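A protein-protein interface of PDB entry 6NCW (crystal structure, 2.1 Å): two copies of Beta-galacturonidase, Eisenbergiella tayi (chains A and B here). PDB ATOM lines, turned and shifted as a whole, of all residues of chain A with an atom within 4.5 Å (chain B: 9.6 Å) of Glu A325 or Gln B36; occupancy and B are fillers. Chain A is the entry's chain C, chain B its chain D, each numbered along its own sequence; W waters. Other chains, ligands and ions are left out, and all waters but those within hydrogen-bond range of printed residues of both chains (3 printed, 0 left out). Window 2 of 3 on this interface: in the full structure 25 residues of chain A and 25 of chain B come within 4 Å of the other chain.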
ATOM      1  N   THR A   4      -2.709   5.970  -2.047  1.00  0.00           N
ATOM      2  CA  THR A   4      -3.422   5.132  -3.005  1.00  0.00           C
ATOM      3  C   THR A   4      -3.014   5.396  -4.458  1.00  0.00           C
ATOM      4  O   THR A   4      -3.544   4.731  -5.355  1.00  0.00           O
ATOM      5  CB  THR A   4      -4.942   5.310  -2.872  1.00  0.00           C
ATOM      6  OG1 THR A   4      -5.276   6.682  -3.096  1.00  0.00           O
ATOM      7  CG2 THR A   4      -5.455   4.898  -1.479  1.00  0.00           C
ATOM      8  N   PRO A 228     -17.273  11.940  -6.772  1.00  0.00           N
ATOM      9  CA  PRO A 228     -15.948  12.387  -6.293  1.00  0.00           C
ATOM     10  C   PRO A 228     -14.866  12.280  -7.366  1.00  0.00           C
ATOM     11  O   PRO A 228     -13.895  11.523  -7.238  1.00  0.00           O
ATOM     12  CB  PRO A 228     -15.706  11.453  -5.095  1.00  0.00           C
ATOM     13  CG  PRO A 228     -16.413  10.173  -5.476  1.00  0.00           C
ATOM     14  CD  PRO A 228     -17.621  10.585  -6.291  1.00  0.00           C
ATOM     15  N   LEU A 230     -11.618  12.940  -9.302  1.00  0.00           N
ATOM     16  CA  LEU A 230     -10.303  13.407  -8.903  1.00  0.00           C
ATOM     17  C   LEU A 230      -9.414  13.515 -10.135  1.00  0.00           C
ATOM     18  O   LEU A 230      -9.564  12.757 -11.091  1.00  0.00           O
ATOM     19  CB  LEU A 230      -9.650  12.455  -7.859  1.00  0.00           C
ATOM     20  CG  LEU A 230     -10.351  12.254  -6.510  1.00  0.00           C
ATOM     21  CD1 LEU A 230      -9.624  11.195  -5.662  1.00  0.00           C
ATOM     22  CD2 LEU A 230     -10.475  13.549  -5.734  1.00  0.00           C
ATOM     23  N   ARG A 250      -3.135  14.665  -6.073  1.00  0.00           N
ATOM     24  CA  ARG A 250      -4.498  14.566  -6.584  1.00  0.00           C
ATOM     25  C   ARG A 250      -5.325  15.715  -6.044  1.00  0.00           C
ATOM     26  O   ARG A 250      -5.165  16.116  -4.888  1.00  0.00           O
ATOM     27  CB  ARG A 250      -5.201  13.263  -6.211  1.00  0.00           C
ATOM     28  CG  ARG A 250      -4.627  12.021  -6.813  1.00  0.00           C
ATOM     29  CD  ARG A 250      -5.621  10.858  -6.729  1.00  0.00           C
ATOM     30  NE  ARG A 250      -6.016  10.580  -5.348  1.00  0.00           N
ATOM     31  CZ  ARG A 250      -6.580   9.446  -4.934  1.00  0.00           C
ATOM     32  NH1 ARG A 250      -6.830   8.452  -5.782  1.00  0.00           N
ATOM     33  NH2 ARG A 250      -6.901   9.307  -3.663  1.00  0.00           N
ATOM     34  N   GLN A 294     -10.307   0.859   5.285  1.00  0.00           N
ATOM     35  CA  GLN A 294     -11.450   0.705   4.395  1.00  0.00           C
ATOM     36  C   GLN A 294     -12.569  -0.088   5.061  1.00  0.00           C
ATOM     37  O   GLN A 294     -13.751   0.167   4.795  1.00  0.00           O
ATOM     38  CB  GLN A 294     -10.996   0.054   3.080  1.00  0.00           C
ATOM     39  CG  GLN A 294     -12.085  -0.092   1.994  1.00  0.00           C
ATOM     40  CD  GLN A 294     -12.799   1.213   1.666  1.00  0.00           C
ATOM     41  OE1 GLN A 294     -12.251   2.296   1.840  1.00  0.00           O
ATOM     42  NE2 GLN A 294     -14.037   1.108   1.186  1.00  0.00           N
ATOM     43  N   LYS A 301     -19.972   4.242   5.956  1.00  0.00           N
ATOM     44  CA  LYS A 301     -20.917   4.449   4.860  1.00  0.00           C
ATOM     45  C   LYS A 301     -22.202   3.651   5.070  1.00  0.00           C
ATOM     46  O   LYS A 301     -23.289   4.137   4.764  1.00  0.00           O
ATOM     47  CB  LYS A 301     -20.273   4.087   3.524  1.00  0.00           C
ATOM     48  CG  LYS A 301     -19.260   5.139   3.078  1.00  0.00           C
ATOM     49  CD  LYS A 301     -18.908   5.030   1.617  1.00  0.00           C
ATOM     50  CE  LYS A 301     -18.272   3.696   1.309  1.00  0.00           C
ATOM     51  NZ  LYS A 301     -17.864   3.615  -0.136  1.00  0.00           N
ATOM     52  N   ASP A 321      -6.717   9.924   1.449  1.00  0.00           N
ATOM     53  CA  ASP A 321      -6.854   9.475   0.063  1.00  0.00           C
ATOM     54  C   ASP A 321      -8.138   8.686  -0.119  1.00  0.00           C
ATOM     55  O   ASP A 321      -8.855   8.866  -1.111  1.00  0.00           O
ATOM     56  CB  ASP A 321      -5.674   8.589  -0.361  1.00  0.00           C
ATOM     57  CG  ASP A 321      -4.405   9.366  -0.692  1.00  0.00           C
ATOM     58  OD1 ASP A 321      -3.343   8.708  -0.768  1.00  0.00           O
ATOM     59  OD2 ASP A 321      -4.445  10.600  -0.864  1.00  0.00           O
ATOM     60  N   LEU A 322      -8.425   7.779   0.822  1.00  0.00           N
ATOM     61  CA  LEU A 322      -9.612   6.944   0.717  1.00  0.00           C
ATOM     62  C   LEU A 322     -10.886   7.768   0.849  1.00  0.00           C
ATOM     63  O   LEU A 322     -11.902   7.428   0.237  1.00  0.00           O
ATOM     64  CB  LEU A 322      -9.558   5.841   1.775  1.00  0.00           C
ATOM     65  CG  LEU A 322      -8.513   4.737   1.527  1.00  0.00           C
ATOM     66  CD1 LEU A 322      -8.366   3.847   2.770  1.00  0.00           C
ATOM     67  CD2 LEU A 322      -8.929   3.926   0.341  1.00  0.00           C
ATOM     68  N   CYS A 323     -10.853   8.846   1.641  1.00  0.00           N
ATOM     69  CA  CYS A 323     -12.007   9.738   1.734  1.00  0.00           C
ATOM     70  C   CYS A 323     -12.198  10.540   0.446  1.00  0.00           C
ATOM     71  O   CYS A 323     -13.338  10.754   0.016  1.00  0.00           O
ATOM     72  CB  CYS A 323     -11.854  10.678   2.929  1.00  0.00           C
ATOM     73  SG  CYS A 323     -11.963   9.848   4.558  1.00  0.00           S
ATOM     74  N   ASP A 324     -11.096  11.004  -0.165  1.00  0.00           N
ATOM     75  CA  ASP A 324     -11.150  11.663  -1.474  1.00  0.00           C
ATOM     76  C   ASP A 324     -11.857  10.791  -2.507  1.00  0.00           C
ATOM     77  O   ASP A 324     -12.777  11.245  -3.187  1.00  0.00           O
ATOM     78  CB  ASP A 324      -9.738  11.987  -1.991  1.00  0.00           C
ATOM     79  CG  ASP A 324      -9.019  13.042  -1.177  1.00  0.00           C
ATOM     80  OD1 ASP A 324      -9.690  13.826  -0.468  1.00  0.00           O
ATOM     81  OD2 ASP A 324      -7.759  13.101  -1.267  1.00  0.00           O
ATOM     82  N   GLU A 325     -11.420   9.530  -2.649  1.00  0.00           N
ATOM     83  CA  GLU A 325     -11.962   8.663  -3.690  1.00  0.00           C
ATOM     84  C   GLU A 325     -13.409   8.289  -3.449  1.00  0.00           C
ATOM     85  O   GLU A 325     -14.086   7.904  -4.403  1.00  0.00           O
ATOM     86  CB  GLU A 325     -11.160   7.361  -3.814  1.00  0.00           C
ATOM     87  CG  GLU A 325      -9.669   7.544  -3.726  1.00  0.00           C
ATOM     88  CD  GLU A 325      -8.877   6.305  -4.119  1.00  0.00           C
ATOM     89  OE1 GLU A 325      -7.664   6.465  -4.401  1.00  0.00           O
ATOM     90  OE2 GLU A 325      -9.453   5.187  -4.161  1.00  0.00           O
ATOM     91  N   GLN A 326     -13.881   8.333  -2.198  1.00  0.00           N
ATOM     92  CA  GLN A 326     -15.229   7.885  -1.857  1.00  0.00           C
ATOM     93  C   GLN A 326     -16.160   9.045  -1.535  1.00  0.00           C
ATOM     94  O   GLN A 326     -17.310   8.817  -1.148  1.00  0.00           O
ATOM     95  CB  GLN A 326     -15.178   6.886  -0.688  1.00  0.00           C
ATOM     96  CG  GLN A 326     -14.488   5.597  -1.111  1.00  0.00           C
ATOM     97  CD  GLN A 326     -14.208   4.636   0.042  1.00  0.00           C
ATOM     98  OE1 GLN A 326     -14.889   3.624   0.200  1.00  0.00           O
ATOM     99  NE2 GLN A 326     -13.184   4.936   0.825  1.00  0.00           N
ATOM    100  N   GLY A 327     -15.692  10.278  -1.698  1.00  0.00           N
ATOM    101  CA  GLY A 327     -16.533  11.443  -1.481  1.00  0.00           C
ATOM    102  C   GLY A 327     -16.962  11.669  -0.047  1.00  0.00           C
ATOM    103  O   GLY A 327     -18.080  12.136   0.190  1.00  0.00           O
ATOM    104  N   SER B  18      -4.241  -3.334  -3.749  1.00  0.00           N
ATOM    105  CA  SER B  18      -4.091  -2.235  -2.789  1.00  0.00           C
ATOM    106  C   SER B  18      -4.809  -0.978  -3.294  1.00  0.00           C
ATOM    107  O   SER B  18      -4.234   0.104  -3.395  1.00  0.00           O
ATOM    108  CB  SER B  18      -2.620  -1.937  -2.484  1.00  0.00           C
ATOM    109  OG  SER B  18      -1.998  -3.022  -1.821  1.00  0.00           O
ATOM    110  N   ALA B  19      -6.103  -1.133  -3.569  1.00  0.00           N
ATOM    111  CA  ALA B  19      -6.879  -0.086  -4.222  1.00  0.00           C
ATOM    112  C   ALA B  19      -8.353  -0.428  -4.132  1.00  0.00           C
ATOM    113  O   ALA B  19      -8.725  -1.573  -3.871  1.00  0.00           O
ATOM    114  CB  ALA B  19      -6.472   0.077  -5.691  1.00  0.00           C
ATOM    115  N   LEU B  20      -9.194   0.577  -4.371  1.00  0.00           N
ATOM    116  CA  LEU B  20     -10.626   0.366  -4.499  1.00  0.00           C
ATOM    117  C   LEU B  20     -10.968   0.012  -5.943  1.00  0.00           C
ATOM    118  O   LEU B  20     -10.563   0.713  -6.879  1.00  0.00           O
ATOM    119  CB  LEU B  20     -11.387   1.619  -4.055  1.00  0.00           C
ATOM    120  CG  LEU B  20     -11.108   2.042  -2.607  1.00  0.00           C
ATOM    121  CD1 LEU B  20     -11.914   3.263  -2.193  1.00  0.00           C
ATOM    122  CD2 LEU B  20     -11.380   0.862  -1.657  1.00  0.00           C
ATOM    123  N   TRP B  21     -11.696  -1.083  -6.125  1.00  0.00           N
ATOM    124  CA  TRP B  21     -12.293  -1.398  -7.412  1.00  0.00           C
ATOM    125  C   TRP B  21     -13.806  -1.255  -7.314  1.00  0.00           C
ATOM    126  O   TRP B  21     -14.380  -1.228  -6.226  1.00  0.00           O
ATOM    127  CB  TRP B  21     -11.970  -2.823  -7.863  1.00  0.00           C
ATOM    128  CG  TRP B  21     -10.536  -3.203  -8.045  1.00  0.00           C
ATOM    129  CD1 TRP B  21      -9.443  -2.700  -7.394  1.00  0.00           C
ATOM    130  CD2 TRP B  21     -10.049  -4.222  -8.922  1.00  0.00           C
ATOM    131  NE1 TRP B  21      -8.307  -3.349  -7.823  1.00  0.00           N
ATOM    132  CE2 TRP B  21      -8.655  -4.294  -8.751  1.00  0.00           C
ATOM    133  CE3 TRP B  21     -10.665  -5.085  -9.839  1.00  0.00           C
ATOM    134  CZ2 TRP B  21      -7.861  -5.169  -9.483  1.00  0.00           C
ATOM    135  CZ3 TRP B  21      -9.878  -5.975 -10.546  1.00  0.00           C
ATOM    136  CH2 TRP B  21      -8.492  -6.014 -10.359  1.00  0.00           C
ATOM    137  N   ASN B  22     -14.457  -1.222  -8.470  1.00  0.00           N
ATOM    138  CA  ASN B  22     -15.916  -1.227  -8.506  1.00  0.00           C
ATOM    139  C   ASN B  22     -16.431  -2.654  -8.364  1.00  0.00           C
ATOM    140  O   ASN B  22     -15.937  -3.575  -9.027  1.00  0.00           O
ATOM    141  CB  ASN B  22     -16.430  -0.612  -9.811  1.00  0.00           C
ATOM    142  CG  ASN B  22     -16.254   0.894  -9.854  1.00  0.00           C
ATOM    143  OD1 ASN B  22     -16.256   1.571  -8.820  1.00  0.00           O
ATOM    144  ND2 ASN B  22     -16.116   1.433 -11.061  1.00  0.00           N
ATOM    145  N   PHE B  23     -17.455  -2.816  -7.527  1.00  0.00           N
ATOM    146  CA  PHE B  23     -17.968  -4.115  -7.128  1.00  0.00           C
ATOM    147  C   PHE B  23     -19.491  -4.120  -7.167  1.00  0.00           C
ATOM    148  O   PHE B  23     -20.130  -3.186  -6.674  1.00  0.00           O
ATOM    149  CB  PHE B  23     -17.483  -4.463  -5.712  1.00  0.00           C
ATOM    150  CG  PHE B  23     -18.051  -5.755  -5.166  1.00  0.00           C
ATOM    151  CD1 PHE B  23     -19.202  -5.750  -4.380  1.00  0.00           C
ATOM    152  CD2 PHE B  23     -17.426  -6.971  -5.439  1.00  0.00           C
ATOM    153  CE1 PHE B  23     -19.716  -6.923  -3.860  1.00  0.00           C
ATOM    154  CE2 PHE B  23     -17.938  -8.156  -4.947  1.00  0.00           C
ATOM    155  CZ  PHE B  23     -19.093  -8.134  -4.143  1.00  0.00           C
ATOM    156  N   HIS B  24     -20.062  -5.182  -7.737  1.00  0.00           N
ATOM    157  CA  HIS B  24     -21.479  -5.482  -7.619  1.00  0.00           C
ATOM    158  C   HIS B  24     -21.665  -6.989  -7.779  1.00  0.00           C
ATOM    159  O   HIS B  24     -20.888  -7.651  -8.474  1.00  0.00           O
ATOM    160  CB  HIS B  24     -22.327  -4.716  -8.654  1.00  0.00           C
ATOM    161  CG  HIS B  24     -21.982  -5.028 -10.073  1.00  0.00           C
ATOM    162  ND1 HIS B  24     -22.548  -6.078 -10.765  1.00  0.00           N
ATOM    163  CD2 HIS B  24     -21.121  -4.433 -10.930  1.00  0.00           C
ATOM    164  CE1 HIS B  24     -22.056  -6.108 -11.990  1.00  0.00           C
ATOM    165  NE2 HIS B  24     -21.186  -5.122 -12.113  1.00  0.00           N
ATOM    166  N   ALA B  33     -26.461  -2.290  -6.708  1.00  0.00           N
ATOM    167  CA  ALA B  33     -25.587  -1.183  -6.345  1.00  0.00           C
ATOM    168  C   ALA B  33     -24.148  -1.495  -6.737  1.00  0.00           C
ATOM    169  O   ALA B  33     -23.654  -2.603  -6.505  1.00  0.00           O
ATOM    170  CB  ALA B  33     -25.673  -0.920  -4.837  1.00  0.00           C
ATOM    171  N   VAL B  34     -23.482  -0.532  -7.349  1.00  0.00           N
ATOM    172  CA  VAL B  34     -22.034  -0.590  -7.502  1.00  0.00           C
ATOM    173  C   VAL B  34     -21.436   0.105  -6.287  1.00  0.00           C
ATOM    174  O   VAL B  34     -21.790   1.247  -5.974  1.00  0.00           O
ATOM    175  CB  VAL B  34     -21.574   0.069  -8.812  1.00  0.00           C
ATOM    176  CG1 VAL B  34     -20.082  -0.135  -9.011  1.00  0.00           C
ATOM    177  CG2 VAL B  34     -22.337  -0.516  -9.992  1.00  0.00           C
ATOM    178  N   ILE B  35     -20.569  -0.592  -5.569  1.00  0.00           N
ATOM    179  CA  ILE B  35     -19.886   0.019  -4.440  1.00  0.00           C
ATOM    180  C   ILE B  35     -18.381   0.004  -4.706  1.00  0.00           C
ATOM    181  O   ILE B  35     -17.885  -0.698  -5.590  1.00  0.00           O
ATOM    182  CB  ILE B  35     -20.245  -0.682  -3.107  1.00  0.00           C
ATOM    183  CG1 ILE B  35     -19.692  -2.094  -3.047  1.00  0.00           C
ATOM    184  CG2 ILE B  35     -21.749  -0.786  -2.964  1.00  0.00           C
ATOM    185  CD1 ILE B  35     -19.224  -2.469  -1.663  1.00  0.00           C
ATOM    186  N   GLN B  36     -17.650   0.803  -3.936  1.00  0.00           N
ATOM    187  CA  GLN B  36     -16.190   0.830  -4.010  1.00  0.00           C
ATOM    188  C   GLN B  36     -15.639  -0.151  -2.980  1.00  0.00           C
ATOM    189  O   GLN B  36     -15.774   0.065  -1.772  1.00  0.00           O
ATOM    190  CB  GLN B  36     -15.669   2.247  -3.786  1.00  0.00           C
ATOM    191  CG  GLN B  36     -15.961   3.171  -4.967  1.00  0.00           C
ATOM    192  CD  GLN B  36     -15.830   4.626  -4.606  1.00  0.00           C
ATOM    193  OE1 GLN B  36     -16.613   5.156  -3.808  1.00  0.00           O
ATOM    194  NE2 GLN B  36     -14.832   5.290  -5.183  1.00  0.00           N
ATOM    195  N   ALA B  37     -15.039  -1.243  -3.455  1.00  0.00           N
ATOM    196  CA  ALA B  37     -14.627  -2.338  -2.597  1.00  0.00           C
ATOM    197  C   ALA B  37     -13.111  -2.467  -2.577  1.00  0.00           C
ATOM    198  O   ALA B  37     -12.456  -2.250  -3.605  1.00  0.00           O
ATOM    199  CB  ALA B  37     -15.228  -3.665  -3.068  1.00  0.00           C
ATOM    200  N   PRO B  38     -12.518  -2.833  -1.441  1.00  0.00           N
ATOM    201  CA  PRO B  38     -11.059  -2.969  -1.398  1.00  0.00           C
ATOM    202  C   PRO B  38     -10.598  -4.255  -2.073  1.00  0.00           C
ATOM    203  O   PRO B  38     -11.252  -5.300  -1.996  1.00  0.00           O
ATOM    204  CB  PRO B  38     -10.750  -2.982   0.102  1.00  0.00           C
ATOM    205  CG  PRO B  38     -11.972  -3.643   0.701  1.00  0.00           C
ATOM    206  CD  PRO B  38     -13.153  -3.134  -0.143  1.00  0.00           C
ATOM    207  N   VAL B  39      -9.450  -4.160  -2.741  1.00  0.00           N
ATOM    208  CA  VAL B  39      -8.754  -5.310  -3.298  1.00  0.00           C
ATOM    209  C   VAL B  39      -7.314  -5.222  -2.810  1.00  0.00           C
ATOM    210  O   VAL B  39      -6.638  -4.226  -3.068  1.00  0.00           O
ATOM    211  CB  VAL B  39      -8.797  -5.347  -4.836  1.00  0.00           C
ATOM    212  CG1 VAL B  39      -7.902  -6.449  -5.367  1.00  0.00           C
ATOM    213  CG2 VAL B  39     -10.231  -5.541  -5.324  1.00  0.00           C
ATOM    214  N   ASN B  45     -16.874  -9.479   4.102  1.00  0.00           N
ATOM    215  CA  ASN B  45     -16.599  -8.386   5.017  1.00  0.00           C
ATOM    216  C   ASN B  45     -17.214  -7.079   4.552  1.00  0.00           C
ATOM    217  O   ASN B  45     -17.071  -6.074   5.256  1.00  0.00           O
ATOM    218  CB  ASN B  45     -15.084  -8.211   5.187  1.00  0.00           C
ATOM    219  CG  ASN B  45     -14.391  -9.518   5.557  1.00  0.00           C
ATOM    220  OD1 ASN B  45     -13.456  -9.932   4.894  1.00  0.00           O
ATOM    221  ND2 ASN B  45     -14.868 -10.178   6.627  1.00  0.00           N
ATOM    222  N   TYR B  46     -17.865  -7.061   3.359  1.00  0.00           N
ATOM    223  CA  TYR B  46     -18.510  -5.781   3.095  1.00  0.00           C
ATOM    224  C   TYR B  46     -19.928  -5.818   3.663  1.00  0.00           C
ATOM    225  O   TYR B  46     -20.582  -6.855   3.603  1.00  0.00           O
ATOM    226  CB  TYR B  46     -18.563  -5.467   1.601  1.00  0.00           C
ATOM    227  CG  TYR B  46     -17.350  -5.844   0.767  1.00  0.00           C
ATOM    228  CD1 TYR B  46     -17.504  -6.102  -0.586  1.00  0.00           C
ATOM    229  CD2 TYR B  46     -16.061  -5.918   1.310  1.00  0.00           C
ATOM    230  CE1 TYR B  46     -16.444  -6.438  -1.375  1.00  0.00           C
ATOM    231  CE2 TYR B  46     -14.969  -6.260   0.513  1.00  0.00           C
ATOM    232  CZ  TYR B  46     -15.182  -6.520  -0.834  1.00  0.00           C
ATOM    233  OH  TYR B  46     -14.162  -6.870  -1.673  1.00  0.00           O
ATOM    234  N   PRO B  47     -20.428  -4.730   4.256  1.00  0.00           N
ATOM    235  CA  PRO B  47     -21.736  -4.799   4.957  1.00  0.00           C
ATOM    236  C   PRO B  47     -22.899  -5.424   4.168  1.00  0.00           C
ATOM    237  O   PRO B  47     -23.673  -6.188   4.748  1.00  0.00           O
ATOM    238  CB  PRO B  47     -21.989  -3.325   5.290  1.00  0.00           C
ATOM    239  CG  PRO B  47     -20.606  -2.805   5.556  1.00  0.00           C
ATOM    240  CD  PRO B  47     -19.744  -3.453   4.498  1.00  0.00           C
ATOM    241  N   ASP B  48     -23.033  -5.164   2.869  1.00  0.00           N
ATOM    242  CA  ASP B  48     -24.194  -5.637   2.113  1.00  0.00           C
ATOM    243  C   ASP B  48     -24.058  -7.060   1.580  1.00  0.00           C
ATOM    244  O   ASP B  48     -25.046  -7.616   1.085  1.00  0.00           O
ATOM    245  CB  ASP B  48     -24.470  -4.688   0.940  1.00  0.00           C
ATOM    246  CG  ASP B  48     -24.720  -3.256   1.409  1.00  0.00           C
ATOM    247  OD1 ASP B  48     -25.649  -3.058   2.224  1.00  0.00           O
ATOM    248  OD2 ASP B  48     -23.958  -2.348   1.006  1.00  0.00           O
ATOM    249  N   SER B  57     -18.814  -9.175  -9.522  1.00  0.00           N
ATOM    250  CA  SER B  57     -17.903  -8.572 -10.490  1.00  0.00           C
ATOM    251  C   SER B  57     -17.023  -7.503  -9.851  1.00  0.00           C
ATOM    252  O   SER B  57     -17.520  -6.610  -9.154  1.00  0.00           O
ATOM    253  CB  SER B  57     -18.676  -7.952 -11.652  1.00  0.00           C
ATOM    254  OG  SER B  57     -17.958  -6.861 -12.188  1.00  0.00           O
ATOM    255  N   TYR B  58     -15.728  -7.573 -10.133  1.00  0.00           N
ATOM    256  CA  TYR B  58     -14.776  -6.532  -9.770  1.00  0.00           C
ATOM    257  C   TYR B  58     -14.212  -5.901 -11.037  1.00  0.00           C
ATOM    258  O   TYR B  58     -13.805  -6.613 -11.957  1.00  0.00           O
ATOM    259  CB  TYR B  58     -13.609  -7.094  -8.956  1.00  0.00           C
ATOM    260  CG  TYR B  58     -13.943  -7.564  -7.550  1.00  0.00           C
ATOM    261  CD1 TYR B  58     -13.593  -6.796  -6.443  1.00  0.00           C
ATOM    262  CD2 TYR B  58     -14.564  -8.786  -7.333  1.00  0.00           C
ATOM    263  CE1 TYR B  58     -13.873  -7.221  -5.162  1.00  0.00           C
ATOM    264  CE2 TYR B  58     -14.840  -9.229  -6.038  1.00  0.00           C
ATOM    265  CZ  TYR B  58     -14.493  -8.437  -4.964  1.00  0.00           C
ATOM    266  OH  TYR B  58     -14.782  -8.854  -3.685  1.00  0.00           O
ATOM    267  N   SER B  59     -14.133  -4.576 -11.070  1.00  0.00           N
ATOM    268  CA  SER B  59     -13.568  -3.946 -12.248  1.00  0.00           C
ATOM    269  C   SER B  59     -12.814  -2.673 -11.879  1.00  0.00           C
ATOM    270  O   SER B  59     -13.125  -2.006 -10.892  1.00  0.00           O
ATOM    271  CB  SER B  59     -14.667  -3.667 -13.291  1.00  0.00           C
ATOM    272  OG  SER B  59     -15.824  -3.099 -12.699  1.00  0.00           O
ATOM    273  N   ARG B  60     -11.798  -2.366 -12.679  1.00  0.00           N
ATOM    274  CA  ARG B  60     -11.106  -1.076 -12.683  1.00  0.00           C
ATOM    275  C   ARG B  60     -10.532  -0.862 -14.085  1.00  0.00           C
ATOM    276  O   ARG B  60     -10.788  -1.648 -15.001  1.00  0.00           O
ATOM    277  CB  ARG B  60      -9.997  -1.025 -11.621  1.00  0.00           C
ATOM    278  CG  ARG B  60      -8.978  -2.150 -11.739  1.00  0.00           C
ATOM    279  CD  ARG B  60      -7.716  -1.820 -10.932  1.00  0.00           C
ATOM    280  NE  ARG B  60      -7.058  -0.628 -11.473  1.00  0.00           N
ATOM    281  CZ  ARG B  60      -6.100   0.058 -10.857  1.00  0.00           C
ATOM    282  NH1 ARG B  60      -5.671  -0.322  -9.658  1.00  0.00           N
ATOM    283  NH2 ARG B  60      -5.568   1.124 -11.446  1.00  0.00           N
HETATM  284  O   HOH W   1      -8.016   3.076  -4.927  1.00  0.00           O
HETATM  285  O   HOH W   2     -19.101   2.871  -2.387  1.00  0.00           O
HETATM  286  O   HOH W   3     -17.580   1.046  -0.172  1.00  0.00           O
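O of Glu A325 lies within hydrogen-bond range of NE2 of Gln B36, at 2.8 Å.
NE2 of Gln A294 is in hydrogen-bond range of OE1 of Gln A326 (2.8 Å). NE2 of Gln A326 is in hydrogen-bond range of O of Leu A322, 2.9 Å away. NZ of Lys A301 lies within hydrogen-bond range of OE1 of Gln A326, at 3.0 Å. The side-chain carboxylate (OE1) of Glu A325 is in salt-bridge range of the guanidinium group (NH1) of Arg A250 (2.6 Å). The backbone carbonyl oxygen (O) of Pro B38 lies within hydrogen-bond range of the side-chain hydroxyl (OH) of Tyr B46, 3.3 Å away. OG1 of Thr A4 lies within hydrogen-bond range of OE1 of Glu A325 (2.7 Å).
Leu B20 touches Gln A294 (CD2 to CD, 3.6 Å). NE2 of Gln A294 touches O of Gln B36, at 3.6 Å. CG of Gln A294 touches CB of Pro B38, 3.7 Å away. Leu B20 touches Leu A322. Leu B20 touches Glu A325 (CD1 to OE2, 3.7 Å). CD1 of Leu B20 touches CD of Gln A326, at 3.5 Å. Gln B36 touches Gln A326 (OE1 to CG, 3.5 Å).
Printed residues of chain B within 4 Å of Glu A325: Leu B20 and Gln B36. No residue of chain B comes within 4 Å of Thr A4. No residue of chain B comes within 4 Å of Asp A324. Gln A326 touches just these residues of chain B: Leu B20 (3.5 Å) and Gln B36 (3.5 Å). Of the printed residues of chain A, Leu B20 touches Gln A294, Leu A322, Glu A325 and Gln A326. Printed residues of chain A within 4 Å of Pro B38: Gln A294. Of the printed residues of chain B, Gln A294 touches Leu B20, Gln B36 and Pro B38. Asn B45 touches none of the printed residues of chain A. Pro A228 touches none of the printed residues of chain B. The nearest residue of chain B that does not touch Glu A325 is Ala B19 (5.7 Å). The nearest residue of chain A that does not touch Gln B36 is Lys A301 (4.2 Å). The nearest printed residue of chain B that does not touch Gln A294 is Ala B37 (5.2 Å).
Of the 13 printed residues of chain A, 4 touch a printed residue of chain B. Hydrophobic or aromatic side chains of chain A that line the printed part of chain B: Leu A322. Hydrophobic or aromatic side chains of chain B within 4 Å of the printed part of chain A: Leu B20 and Pro B38. Among the printed residues, no Asp or Glu carboxylate lies within 4 Å of a Lys or Arg side-chain nitrogen of the other chain.
No position is printed for both chains.
Water W3 bridges the side-chain amino group (NZ) of Lys A301 (2.6 Å) and the backbone carbonyl oxygen (O) of Gln B36 (2.6 Å). Water W1 bridges OE2 of Glu A325 (2.7 Å) and N of Leu B20 (2.8 Å). Water W2 lies within hydrogen-bond range of NZ of Lys A301 (2.7 Å) and N of Gln B36 (3.0 Å).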
